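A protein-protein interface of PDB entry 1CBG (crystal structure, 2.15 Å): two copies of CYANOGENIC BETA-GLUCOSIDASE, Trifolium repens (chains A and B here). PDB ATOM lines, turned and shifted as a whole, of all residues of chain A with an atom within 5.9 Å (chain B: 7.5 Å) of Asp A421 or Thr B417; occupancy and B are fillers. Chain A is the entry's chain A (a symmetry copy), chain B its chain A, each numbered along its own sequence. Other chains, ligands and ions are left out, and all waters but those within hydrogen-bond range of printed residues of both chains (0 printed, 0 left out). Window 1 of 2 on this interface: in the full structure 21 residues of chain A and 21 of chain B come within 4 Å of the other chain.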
ATOM      1  N   PHE A  11     -14.573  25.207  35.658  1.00  0.00           N
ATOM      2  CA  PHE A  11     -14.224  23.791  35.742  1.00  0.00           C
ATOM      3  C   PHE A  11     -13.973  23.386  37.197  1.00  0.00           C
ATOM      4  O   PHE A  11     -14.326  22.264  37.592  1.00  0.00           O
ATOM      5  CB  PHE A  11     -13.011  23.465  34.884  1.00  0.00           C
ATOM      6  CG  PHE A  11     -12.655  22.013  34.787  1.00  0.00           C
ATOM      7  CD1 PHE A  11     -13.411  21.166  33.982  1.00  0.00           C
ATOM      8  CD2 PHE A  11     -11.556  21.508  35.481  1.00  0.00           C
ATOM      9  CE1 PHE A  11     -13.080  19.829  33.863  1.00  0.00           C
ATOM     10  CE2 PHE A  11     -11.214  20.157  35.373  1.00  0.00           C
ATOM     11  CZ  PHE A  11     -11.986  19.315  34.561  1.00  0.00           C
ATOM     12  N   ILE A 372     -19.546   3.641  28.927  1.00  0.00           N
ATOM     13  CA  ILE A 372     -19.660   4.888  29.709  1.00  0.00           C
ATOM     14  C   ILE A 372     -20.995   5.597  29.543  1.00  0.00           C
ATOM     15  O   ILE A 372     -21.302   6.234  28.507  1.00  0.00           O
ATOM     16  CB  ILE A 372     -18.426   5.811  29.371  1.00  0.00           C
ATOM     17  CG1 ILE A 372     -17.122   5.000  29.552  1.00  0.00           C
ATOM     18  CG2 ILE A 372     -18.402   7.127  30.189  1.00  0.00           C
ATOM     19  CD1 ILE A 372     -15.847   5.588  28.878  1.00  0.00           C
ATOM     20  N   ASP A 416      -4.017  11.398  31.188  1.00  0.00           N
ATOM     21  CA  ASP A 416      -5.259  10.642  31.310  1.00  0.00           C
ATOM     22  C   ASP A 416      -6.484  11.518  31.533  1.00  0.00           C
ATOM     23  O   ASP A 416      -7.314  11.361  32.433  1.00  0.00           O
ATOM     24  CB  ASP A 416      -5.096   9.515  32.359  1.00  0.00           C
ATOM     25  CG  ASP A 416      -5.092   9.953  33.812  1.00  0.00           C
ATOM     26  OD1 ASP A 416      -4.791  11.125  34.114  1.00  0.00           O
ATOM     27  OD2 ASP A 416      -5.471   9.127  34.667  1.00  0.00           O
ATOM     28  N   THR A 417      -6.762  12.343  30.494  1.00  0.00           N
ATOM     29  CA  THR A 417      -7.931  13.229  30.427  1.00  0.00           C
ATOM     30  C   THR A 417      -9.216  12.440  30.325  1.00  0.00           C
ATOM     31  O   THR A 417     -10.169  12.856  31.026  1.00  0.00           O
ATOM     32  CB  THR A 417      -7.800  14.479  29.464  1.00  0.00           C
ATOM     33  OG1 THR A 417      -7.425  14.040  28.145  1.00  0.00           O
ATOM     34  CG2 THR A 417      -6.805  15.533  29.959  1.00  0.00           C
ATOM     35  N   PRO A 418      -9.356  11.302  29.650  1.00  0.00           N
ATOM     36  CA  PRO A 418     -10.587  10.505  29.654  1.00  0.00           C
ATOM     37  C   PRO A 418     -11.070  10.046  31.032  1.00  0.00           C
ATOM     38  O   PRO A 418     -12.294   9.912  31.277  1.00  0.00           O
ATOM     39  CB  PRO A 418     -10.289   9.271  28.800  1.00  0.00           C
ATOM     40  CG  PRO A 418      -9.182   9.703  27.874  1.00  0.00           C
ATOM     41  CD  PRO A 418      -8.383  10.673  28.740  1.00  0.00           C
ATOM     42  N   ARG A 419     -10.184   9.765  31.978  1.00  0.00           N
ATOM     43  CA  ARG A 419     -10.427   9.365  33.370  1.00  0.00           C
ATOM     44  C   ARG A 419     -10.990  10.572  34.118  1.00  0.00           C
ATOM     45  O   ARG A 419     -11.966  10.461  34.869  1.00  0.00           O
ATOM     46  CB  ARG A 419      -9.161   8.828  34.063  1.00  0.00           C
ATOM     47  CG  ARG A 419      -9.325   8.422  35.528  1.00  0.00           C
ATOM     48  CD  ARG A 419      -8.181   7.647  36.083  1.00  0.00           C
ATOM     49  NE  ARG A 419      -8.062   6.310  35.544  1.00  0.00           N
ATOM     50  CZ  ARG A 419      -7.170   5.875  34.662  1.00  0.00           C
ATOM     51  NH1 ARG A 419      -6.196   6.629  34.137  1.00  0.00           N
ATOM     52  NH2 ARG A 419      -7.255   4.603  34.267  1.00  0.00           N
ATOM     53  N   ILE A 420     -10.460  11.774  33.877  1.00  0.00           N
ATOM     54  CA  ILE A 420     -10.951  13.036  34.472  1.00  0.00           C
ATOM     55  C   ILE A 420     -12.403  13.222  34.016  1.00  0.00           C
ATOM     56  O   ILE A 420     -13.307  13.478  34.836  1.00  0.00           O
ATOM     57  CB  ILE A 420     -10.036  14.282  34.223  1.00  0.00           C
ATOM     58  CG1 ILE A 420      -8.651  14.060  34.872  1.00  0.00           C
ATOM     59  CG2 ILE A 420     -10.688  15.606  34.710  1.00  0.00           C
ATOM     60  CD1 ILE A 420      -7.595  15.181  34.735  1.00  0.00           C
ATOM     61  N   ASP A 421     -12.674  13.061  32.719  1.00  0.00           N
ATOM     62  CA  ASP A 421     -14.006  13.109  32.122  1.00  0.00           C
ATOM     63  C   ASP A 421     -14.904  12.117  32.883  1.00  0.00           C
ATOM     64  O   ASP A 421     -16.004  12.524  33.287  1.00  0.00           O
ATOM     65  CB  ASP A 421     -13.967  12.793  30.619  1.00  0.00           C
ATOM     66  CG  ASP A 421     -15.330  12.500  30.027  1.00  0.00           C
ATOM     67  OD1 ASP A 421     -16.296  13.214  30.289  1.00  0.00           O
ATOM     68  OD2 ASP A 421     -15.508  11.494  29.326  1.00  0.00           O
ATOM     69  N   TYR A 422     -14.498  10.862  33.011  1.00  0.00           N
ATOM     70  CA  TYR A 422     -15.249   9.822  33.721  1.00  0.00           C
ATOM     71  C   TYR A 422     -15.581  10.220  35.162  1.00  0.00           C
ATOM     72  O   TYR A 422     -16.772  10.126  35.561  1.00  0.00           O
ATOM     73  CB  TYR A 422     -14.513   8.465  33.672  1.00  0.00           C
ATOM     74  CG  TYR A 422     -15.342   7.286  34.152  1.00  0.00           C
ATOM     75  CD1 TYR A 422     -15.528   7.027  35.515  1.00  0.00           C
ATOM     76  CD2 TYR A 422     -15.932   6.416  33.227  1.00  0.00           C
ATOM     77  CE1 TYR A 422     -16.296   5.972  35.973  1.00  0.00           C
ATOM     78  CE2 TYR A 422     -16.689   5.332  33.657  1.00  0.00           C
ATOM     79  CZ  TYR A 422     -16.857   5.104  35.051  1.00  0.00           C
ATOM     80  OH  TYR A 422     -17.619   4.050  35.474  1.00  0.00           O
ATOM     81  N   TYR A 423     -14.627  10.634  35.971  1.00  0.00           N
ATOM     82  CA  TYR A 423     -14.935  11.023  37.358  1.00  0.00           C
ATOM     83  C   TYR A 423     -15.796  12.259  37.434  1.00  0.00           C
ATOM     84  O   TYR A 423     -16.713  12.217  38.280  1.00  0.00           O
ATOM     85  CB  TYR A 423     -13.664  11.107  38.224  1.00  0.00           C
ATOM     86  CG  TYR A 423     -13.116   9.742  38.593  1.00  0.00           C
ATOM     87  CD1 TYR A 423     -13.865   8.823  39.340  1.00  0.00           C
ATOM     88  CD2 TYR A 423     -11.832   9.367  38.173  1.00  0.00           C
ATOM     89  CE1 TYR A 423     -13.367   7.560  39.665  1.00  0.00           C
ATOM     90  CE2 TYR A 423     -11.306   8.116  38.497  1.00  0.00           C
ATOM     91  CZ  TYR A 423     -12.083   7.224  39.236  1.00  0.00           C
ATOM     92  OH  TYR A 423     -11.567   6.006  39.552  1.00  0.00           O
ATOM     93  N   TYR A 424     -15.585  13.289  36.628  1.00  0.00           N
ATOM     94  CA  TYR A 424     -16.390  14.520  36.670  1.00  0.00           C
ATOM     95  C   TYR A 424     -17.890  14.301  36.510  1.00  0.00           C
ATOM     96  O   TYR A 424     -18.690  14.776  37.353  1.00  0.00           O
ATOM     97  CB  TYR A 424     -15.865  15.545  35.638  1.00  0.00           C
ATOM     98  CG  TYR A 424     -16.124  17.005  35.921  1.00  0.00           C
ATOM     99  CD1 TYR A 424     -17.374  17.613  35.788  1.00  0.00           C
ATOM    100  CD2 TYR A 424     -15.056  17.810  36.338  1.00  0.00           C
ATOM    101  CE1 TYR A 424     -17.557  18.972  36.048  1.00  0.00           C
ATOM    102  CE2 TYR A 424     -15.223  19.167  36.605  1.00  0.00           C
ATOM    103  CZ  TYR A 424     -16.484  19.752  36.459  1.00  0.00           C
ATOM    104  OH  TYR A 424     -16.644  21.092  36.734  1.00  0.00           O
ATOM    105  N   ARG A 425     -18.322  13.603  35.471  1.00  0.00           N
ATOM    106  CA  ARG A 425     -19.725  13.320  35.157  1.00  0.00           C
ATOM    107  C   ARG A 425     -20.352  12.317  36.118  1.00  0.00           C
ATOM    108  O   ARG A 425     -21.531  12.481  36.499  1.00  0.00           O
ATOM    109  CB  ARG A 425     -19.908  12.888  33.696  1.00  0.00           C
ATOM    110  CG  ARG A 425     -19.424  13.940  32.683  1.00  0.00           C
ATOM    111  CD  ARG A 425     -19.885  13.577  31.307  1.00  0.00           C
ATOM    112  NE  ARG A 425     -19.070  12.554  30.655  1.00  0.00           N
ATOM    113  CZ  ARG A 425     -19.563  11.687  29.752  1.00  0.00           C
ATOM    114  NH1 ARG A 425     -20.843  11.680  29.379  1.00  0.00           N
ATOM    115  NH2 ARG A 425     -18.784  10.767  29.173  1.00  0.00           N
ATOM    116  N   HIS A 426     -19.599  11.312  36.549  1.00  0.00           N
ATOM    117  CA  HIS A 426     -20.170  10.336  37.525  1.00  0.00           C
ATOM    118  C   HIS A 426     -20.421  11.019  38.861  1.00  0.00           C
ATOM    119  O   HIS A 426     -21.494  10.851  39.446  1.00  0.00           O
ATOM    120  CB  HIS A 426     -19.325   9.052  37.668  1.00  0.00           C
ATOM    121  CG  HIS A 426     -19.573   8.124  36.506  1.00  0.00           C
ATOM    122  ND1 HIS A 426     -18.971   8.248  35.279  1.00  0.00           N
ATOM    123  CD2 HIS A 426     -20.374   7.040  36.435  1.00  0.00           C
ATOM    124  CE1 HIS A 426     -19.423   7.279  34.499  1.00  0.00           C
ATOM    125  NE2 HIS A 426     -20.263   6.523  35.173  1.00  0.00           N
ATOM    126  N   ARG B 400     -14.983  17.498  17.963  1.00  0.00           N
ATOM    127  CA  ARG B 400     -15.793  16.284  18.145  1.00  0.00           C
ATOM    128  C   ARG B 400     -17.253  16.651  18.424  1.00  0.00           C
ATOM    129  O   ARG B 400     -17.508  17.861  18.605  1.00  0.00           O
ATOM    130  CB  ARG B 400     -15.293  15.394  19.288  1.00  0.00           C
ATOM    131  CG  ARG B 400     -15.373  15.968  20.716  1.00  0.00           C
ATOM    132  CD  ARG B 400     -15.433  14.872  21.736  1.00  0.00           C
ATOM    133  NE  ARG B 400     -16.724  14.199  21.763  1.00  0.00           N
ATOM    134  CZ  ARG B 400     -16.953  12.942  22.178  1.00  0.00           C
ATOM    135  NH1 ARG B 400     -16.045  12.103  22.649  1.00  0.00           N
ATOM    136  NH2 ARG B 400     -18.197  12.458  22.126  1.00  0.00           N
ATOM    137  N   SER B 413     -26.811  18.977  29.571  1.00  0.00           N
ATOM    138  CA  SER B 413     -26.356  19.263  28.200  1.00  0.00           C
ATOM    139  C   SER B 413     -25.102  20.129  28.189  1.00  0.00           C
ATOM    140  O   SER B 413     -24.256  19.974  27.284  1.00  0.00           O
ATOM    141  CB  SER B 413     -27.495  19.887  27.391  1.00  0.00           C
ATOM    142  OG  SER B 413     -28.415  18.914  26.927  1.00  0.00           O
ATOM    143  N   LEU B 414     -24.896  21.020  29.141  1.00  0.00           N
ATOM    144  CA  LEU B 414     -23.722  21.876  29.248  1.00  0.00           C
ATOM    145  C   LEU B 414     -22.498  21.189  29.842  1.00  0.00           C
ATOM    146  O   LEU B 414     -21.379  21.769  29.729  1.00  0.00           O
ATOM    147  CB  LEU B 414     -24.125  23.175  29.975  1.00  0.00           C
ATOM    148  CG  LEU B 414     -25.280  24.025  29.481  1.00  0.00           C
ATOM    149  CD1 LEU B 414     -25.385  25.325  30.287  1.00  0.00           C
ATOM    150  CD2 LEU B 414     -25.102  24.389  28.003  1.00  0.00           C
ATOM    151  N   LEU B 415     -22.576  20.004  30.426  1.00  0.00           N
ATOM    152  CA  LEU B 415     -21.421  19.304  31.008  1.00  0.00           C
ATOM    153  C   LEU B 415     -20.691  18.422  29.989  1.00  0.00           C
ATOM    154  O   LEU B 415     -20.669  17.180  30.078  1.00  0.00           O
ATOM    155  CB  LEU B 415     -21.870  18.502  32.228  1.00  0.00           C
ATOM    156  CG  LEU B 415     -22.272  19.037  33.563  1.00  0.00           C
ATOM    157  CD1 LEU B 415     -22.037  17.908  34.590  1.00  0.00           C
ATOM    158  CD2 LEU B 415     -21.479  20.254  34.029  1.00  0.00           C
ATOM    159  N   ASP B 416     -20.039  19.061  29.038  1.00  0.00           N
ATOM    160  CA  ASP B 416     -19.310  18.464  27.923  1.00  0.00           C
ATOM    161  C   ASP B 416     -17.826  18.272  28.202  1.00  0.00           C
ATOM    162  O   ASP B 416     -16.910  18.652  27.466  1.00  0.00           O
ATOM    163  CB  ASP B 416     -19.606  19.241  26.618  1.00  0.00           C
ATOM    164  CG  ASP B 416     -18.930  20.593  26.479  1.00  0.00           C
ATOM    165  OD1 ASP B 416     -18.550  21.213  27.492  1.00  0.00           O
ATOM    166  OD2 ASP B 416     -18.706  21.013  25.325  1.00  0.00           O
ATOM    167  N   THR B 417     -17.568  17.395  29.203  1.00  0.00           N
ATOM    168  CA  THR B 417     -16.221  16.975  29.612  1.00  0.00           C
ATOM    169  C   THR B 417     -15.546  16.158  28.535  1.00  0.00           C
ATOM    170  O   THR B 417     -14.337  16.418  28.330  1.00  0.00           O
ATOM    171  CB  THR B 417     -16.085  16.429  31.092  1.00  0.00           C
ATOM    172  OG1 THR B 417     -17.030  15.366  31.308  1.00  0.00           O
ATOM    173  CG2 THR B 417     -16.270  17.509  32.164  1.00  0.00           C
ATOM    174  N   PRO B 418     -16.167  15.292  27.739  1.00  0.00           N
ATOM    175  CA  PRO B 418     -15.505  14.591  26.634  1.00  0.00           C
ATOM    176  C   PRO B 418     -14.856  15.488  25.579  1.00  0.00           C
ATOM    177  O   PRO B 418     -13.821  15.125  24.968  1.00  0.00           O
ATOM    178  CB  PRO B 418     -16.592  13.748  25.963  1.00  0.00           C
ATOM    179  CG  PRO B 418     -17.621  13.521  27.040  1.00  0.00           C
ATOM    180  CD  PRO B 418     -17.559  14.819  27.840  1.00  0.00           C
ATOM    181  N   ARG B 419     -15.403  16.660  25.286  1.00  0.00           N
ATOM    182  CA  ARG B 419     -14.921  17.690  24.357  1.00  0.00           C
ATOM    183  C   ARG B 419     -13.662  18.315  24.955  1.00  0.00           C
ATOM    184  O   ARG B 419     -12.655  18.509  24.264  1.00  0.00           O
ATOM    185  CB  ARG B 419     -15.983  18.765  24.058  1.00  0.00           C
ATOM    186  CG  ARG B 419     -15.544  19.893  23.124  1.00  0.00           C
ATOM    187  CD  ARG B 419     -16.658  20.747  22.627  1.00  0.00           C
ATOM    188  NE  ARG B 419     -17.539  20.079  21.694  1.00  0.00           N
ATOM    189  CZ  ARG B 419     -18.767  19.631  21.927  1.00  0.00           C
ATOM    190  NH1 ARG B 419     -19.407  19.754  23.096  1.00  0.00           N
ATOM    191  NH2 ARG B 419     -19.401  19.008  20.932  1.00  0.00           N
ATOM    192  N   ILE B 420     -13.639  18.570  26.266  1.00  0.00           N
ATOM    193  CA  ILE B 420     -12.465  19.105  26.990  1.00  0.00           C
ATOM    194  C   ILE B 420     -11.330  18.087  26.835  1.00  0.00           C
ATOM    195  O   ILE B 420     -10.193  18.443  26.464  1.00  0.00           O
ATOM    196  CB  ILE B 420     -12.744  19.535  28.470  1.00  0.00           C
ATOM    197  CG1 ILE B 420     -13.777  20.684  28.501  1.00  0.00           C
ATOM    198  CG2 ILE B 420     -11.445  19.915  29.233  1.00  0.00           C
ATOM    199  CD1 ILE B 420     -14.192  21.252  29.878  1.00  0.00           C
ATOM    200  N   ASP B 421     -11.607  16.803  27.071  1.00  0.00           N
ATOM    201  CA  ASP B 421     -10.680  15.690  26.886  1.00  0.00           C
ATOM    202  C   ASP B 421     -10.131  15.762  25.449  1.00  0.00           C
ATOM    203  O   ASP B 421      -8.902  15.695  25.295  1.00  0.00           O
ATOM    204  CB  ASP B 421     -11.353  14.338  27.164  1.00  0.00           C
ATOM    205  CG  ASP B 421     -10.551  13.151  26.669  1.00  0.00           C
ATOM    206  OD1 ASP B 421      -9.342  13.078  26.878  1.00  0.00           O
ATOM    207  OD2 ASP B 421     -11.090  12.270  25.985  1.00  0.00           O
ATOM    208  N   TYR B 422     -10.991  15.821  24.443  1.00  0.00           N
ATOM    209  CA  TYR B 422     -10.603  15.906  23.032  1.00  0.00           C
ATOM    210  C   TYR B 422      -9.671  17.089  22.751  1.00  0.00           C
ATOM    211  O   TYR B 422      -8.595  16.882  22.131  1.00  0.00           O
ATOM    212  CB  TYR B 422     -11.842  15.940  22.110  1.00  0.00           C
ATOM    213  CG  TYR B 422     -11.528  15.763  20.634  1.00  0.00           C
ATOM    214  CD1 TYR B 422     -11.038  16.820  19.856  1.00  0.00           C
ATOM    215  CD2 TYR B 422     -11.738  14.527  20.013  1.00  0.00           C
ATOM    216  CE1 TYR B 422     -10.727  16.675  18.517  1.00  0.00           C
ATOM    217  CE2 TYR B 422     -11.457  14.356  18.661  1.00  0.00           C
ATOM    218  CZ  TYR B 422     -10.958  15.453  17.905  1.00  0.00           C
ATOM    219  OH  TYR B 422     -10.663  15.280  16.581  1.00  0.00           O
ATOM    220  N   TYR B 423     -10.007  18.303  23.138  1.00  0.00           N
ATOM    221  CA  TYR B 423      -9.117  19.447  22.876  1.00  0.00           C
ATOM    222  C   TYR B 423      -7.820  19.357  23.643  1.00  0.00           C
ATOM    223  O   TYR B 423      -6.799  19.673  22.997  1.00  0.00           O
ATOM    224  CB  TYR B 423      -9.845  20.791  23.060  1.00  0.00           C
ATOM    225  CG  TYR B 423     -10.792  21.103  21.918  1.00  0.00           C
ATOM    226  CD1 TYR B 423     -10.339  21.244  20.600  1.00  0.00           C
ATOM    227  CD2 TYR B 423     -12.164  21.246  22.167  1.00  0.00           C
ATOM    228  CE1 TYR B 423     -11.214  21.515  19.546  1.00  0.00           C
ATOM    229  CE2 TYR B 423     -13.058  21.531  21.133  1.00  0.00           C
ATOM    230  CZ  TYR B 423     -12.571  21.657  19.832  1.00  0.00           C
ATOM    231  OH  TYR B 423     -13.444  21.936  18.827  1.00  0.00           O
ATOM    232  N   LEU B 479     -19.465  23.905  29.260  1.00  0.00           N
ATOM    233  CA  LEU B 479     -18.272  23.896  30.137  1.00  0.00           C
ATOM    234  C   LEU B 479     -16.978  24.080  29.362  1.00  0.00           C
ATOM    235  O   LEU B 479     -16.045  24.791  29.819  1.00  0.00           O
ATOM    236  CB  LEU B 479     -18.353  22.628  30.990  1.00  0.00           C
ATOM    237  CG  LEU B 479     -17.328  22.456  32.096  1.00  0.00           C
ATOM    238  CD1 LEU B 479     -17.520  23.476  33.204  1.00  0.00           C
ATOM    239  CD2 LEU B 479     -17.498  21.024  32.632  1.00  0.00           C
ATOM    240  N   SER B 480     -16.856  23.489  28.176  1.00  0.00           N
ATOM    241  CA  SER B 480     -15.743  23.604  27.239  1.00  0.00           C
ATOM    242  C   SER B 480     -15.500  25.045  26.772  1.00  0.00           C
ATOM    243  O   SER B 480     -14.311  25.347  26.487  1.00  0.00           O
ATOM    244  CB  SER B 480     -15.927  22.734  25.991  1.00  0.00           C
ATOM    245  OG  SER B 480     -17.089  23.146  25.289  1.00  0.00           O
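The backbone nitrogen of Pro B418 lies close to the side-chain carboxylate of Asp A421 (3.3 Å). The backbone nitrogen (N) of Pro A418 sits close to the side-chain carboxylate (OD1) of Asp B421, 3.3 Å away. OD1 of Asp A421 sits at hydrogen-bond distance from OG1 of Thr B417 (2.5 Å). OG1 of Thr A417 sits at hydrogen-bond distance from OD1 of Asp B421, at 2.5 Å.
The side-chain carboxylate (OD1) of Asp A421 is in salt-bridge range of the guanidinium group (NE) of Arg A425 (2.9 Å). O of Leu B414 is in hydrogen-bond range of N of Leu B479, at 2.9 Å. The backbone carbonyl oxygen (O) of Phe A11 lies within hydrogen-bond range of the side-chain hydroxyl (OH) of Tyr A424 (2.7 Å). The backbone NH (N) of Leu B479 is in hydrogen-bond range of the side-chain carboxylate (OD1) of Asp B416 (3.3 Å).
Among the printed residues, pairs that only touch across the chains: Arg A425 with Thr B417 (3.1 Å), Arg A425 with Pro B418 (3.7 Å), Tyr A424 with Thr B417 (3.8 Å), Arg A425 with Leu B415 (3.9 Å) and Tyr A424 with Leu B479 (3.99 Å).
Of chain B, only Thr B417 (2.5 Å) and Pro B418 (3.2 Å) come within 4 Å of Asp A421. Thr B417 touches just these residues of chain A: Asp A421, Tyr A424 and Arg A425. Of the printed residues of chain B, Pro A418 touches Asp B421. Of the printed residues of chain B, Arg A425 touches Leu B415 (3.9 Å), Thr B417 (3.1 Å) and Pro B418 (3.7 Å). Printed residues of chain A within 4 Å of Pro B418: Asp A421 and Arg A425. Of the printed residues of chain A, Leu B415 touches Arg A425 (3.9 Å). Of the printed residues of chain A, Leu B479 touches Tyr A424 (3.99 Å). The nearest residue of chain B that does not touch Asp A421 is Asp B421 (4.6 Å). The nearest residue of chain A that does not touch Thr B417 is Phe A11 (4.3 Å).
Printed residues of chain A that touch a printed residue of chain B: Thr A417, Pro A418, Asp A421, Tyr A424 and Arg A425. Hydrophobic or aromatic side chains of chain A that line the printed part of chain B: Pro A418 and Tyr A424. Of the 14 printed residues of chain B, 5 touch a printed residue of chain A. Among the printed residues, 9 pairs touch across the chains.
Thr A417 touches Asp B421, and with the chains exchanged Asp A421 touches Thr B417. Pro A418 touches Asp B421, and with the chains exchanged Asp A421 touches Pro B418.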
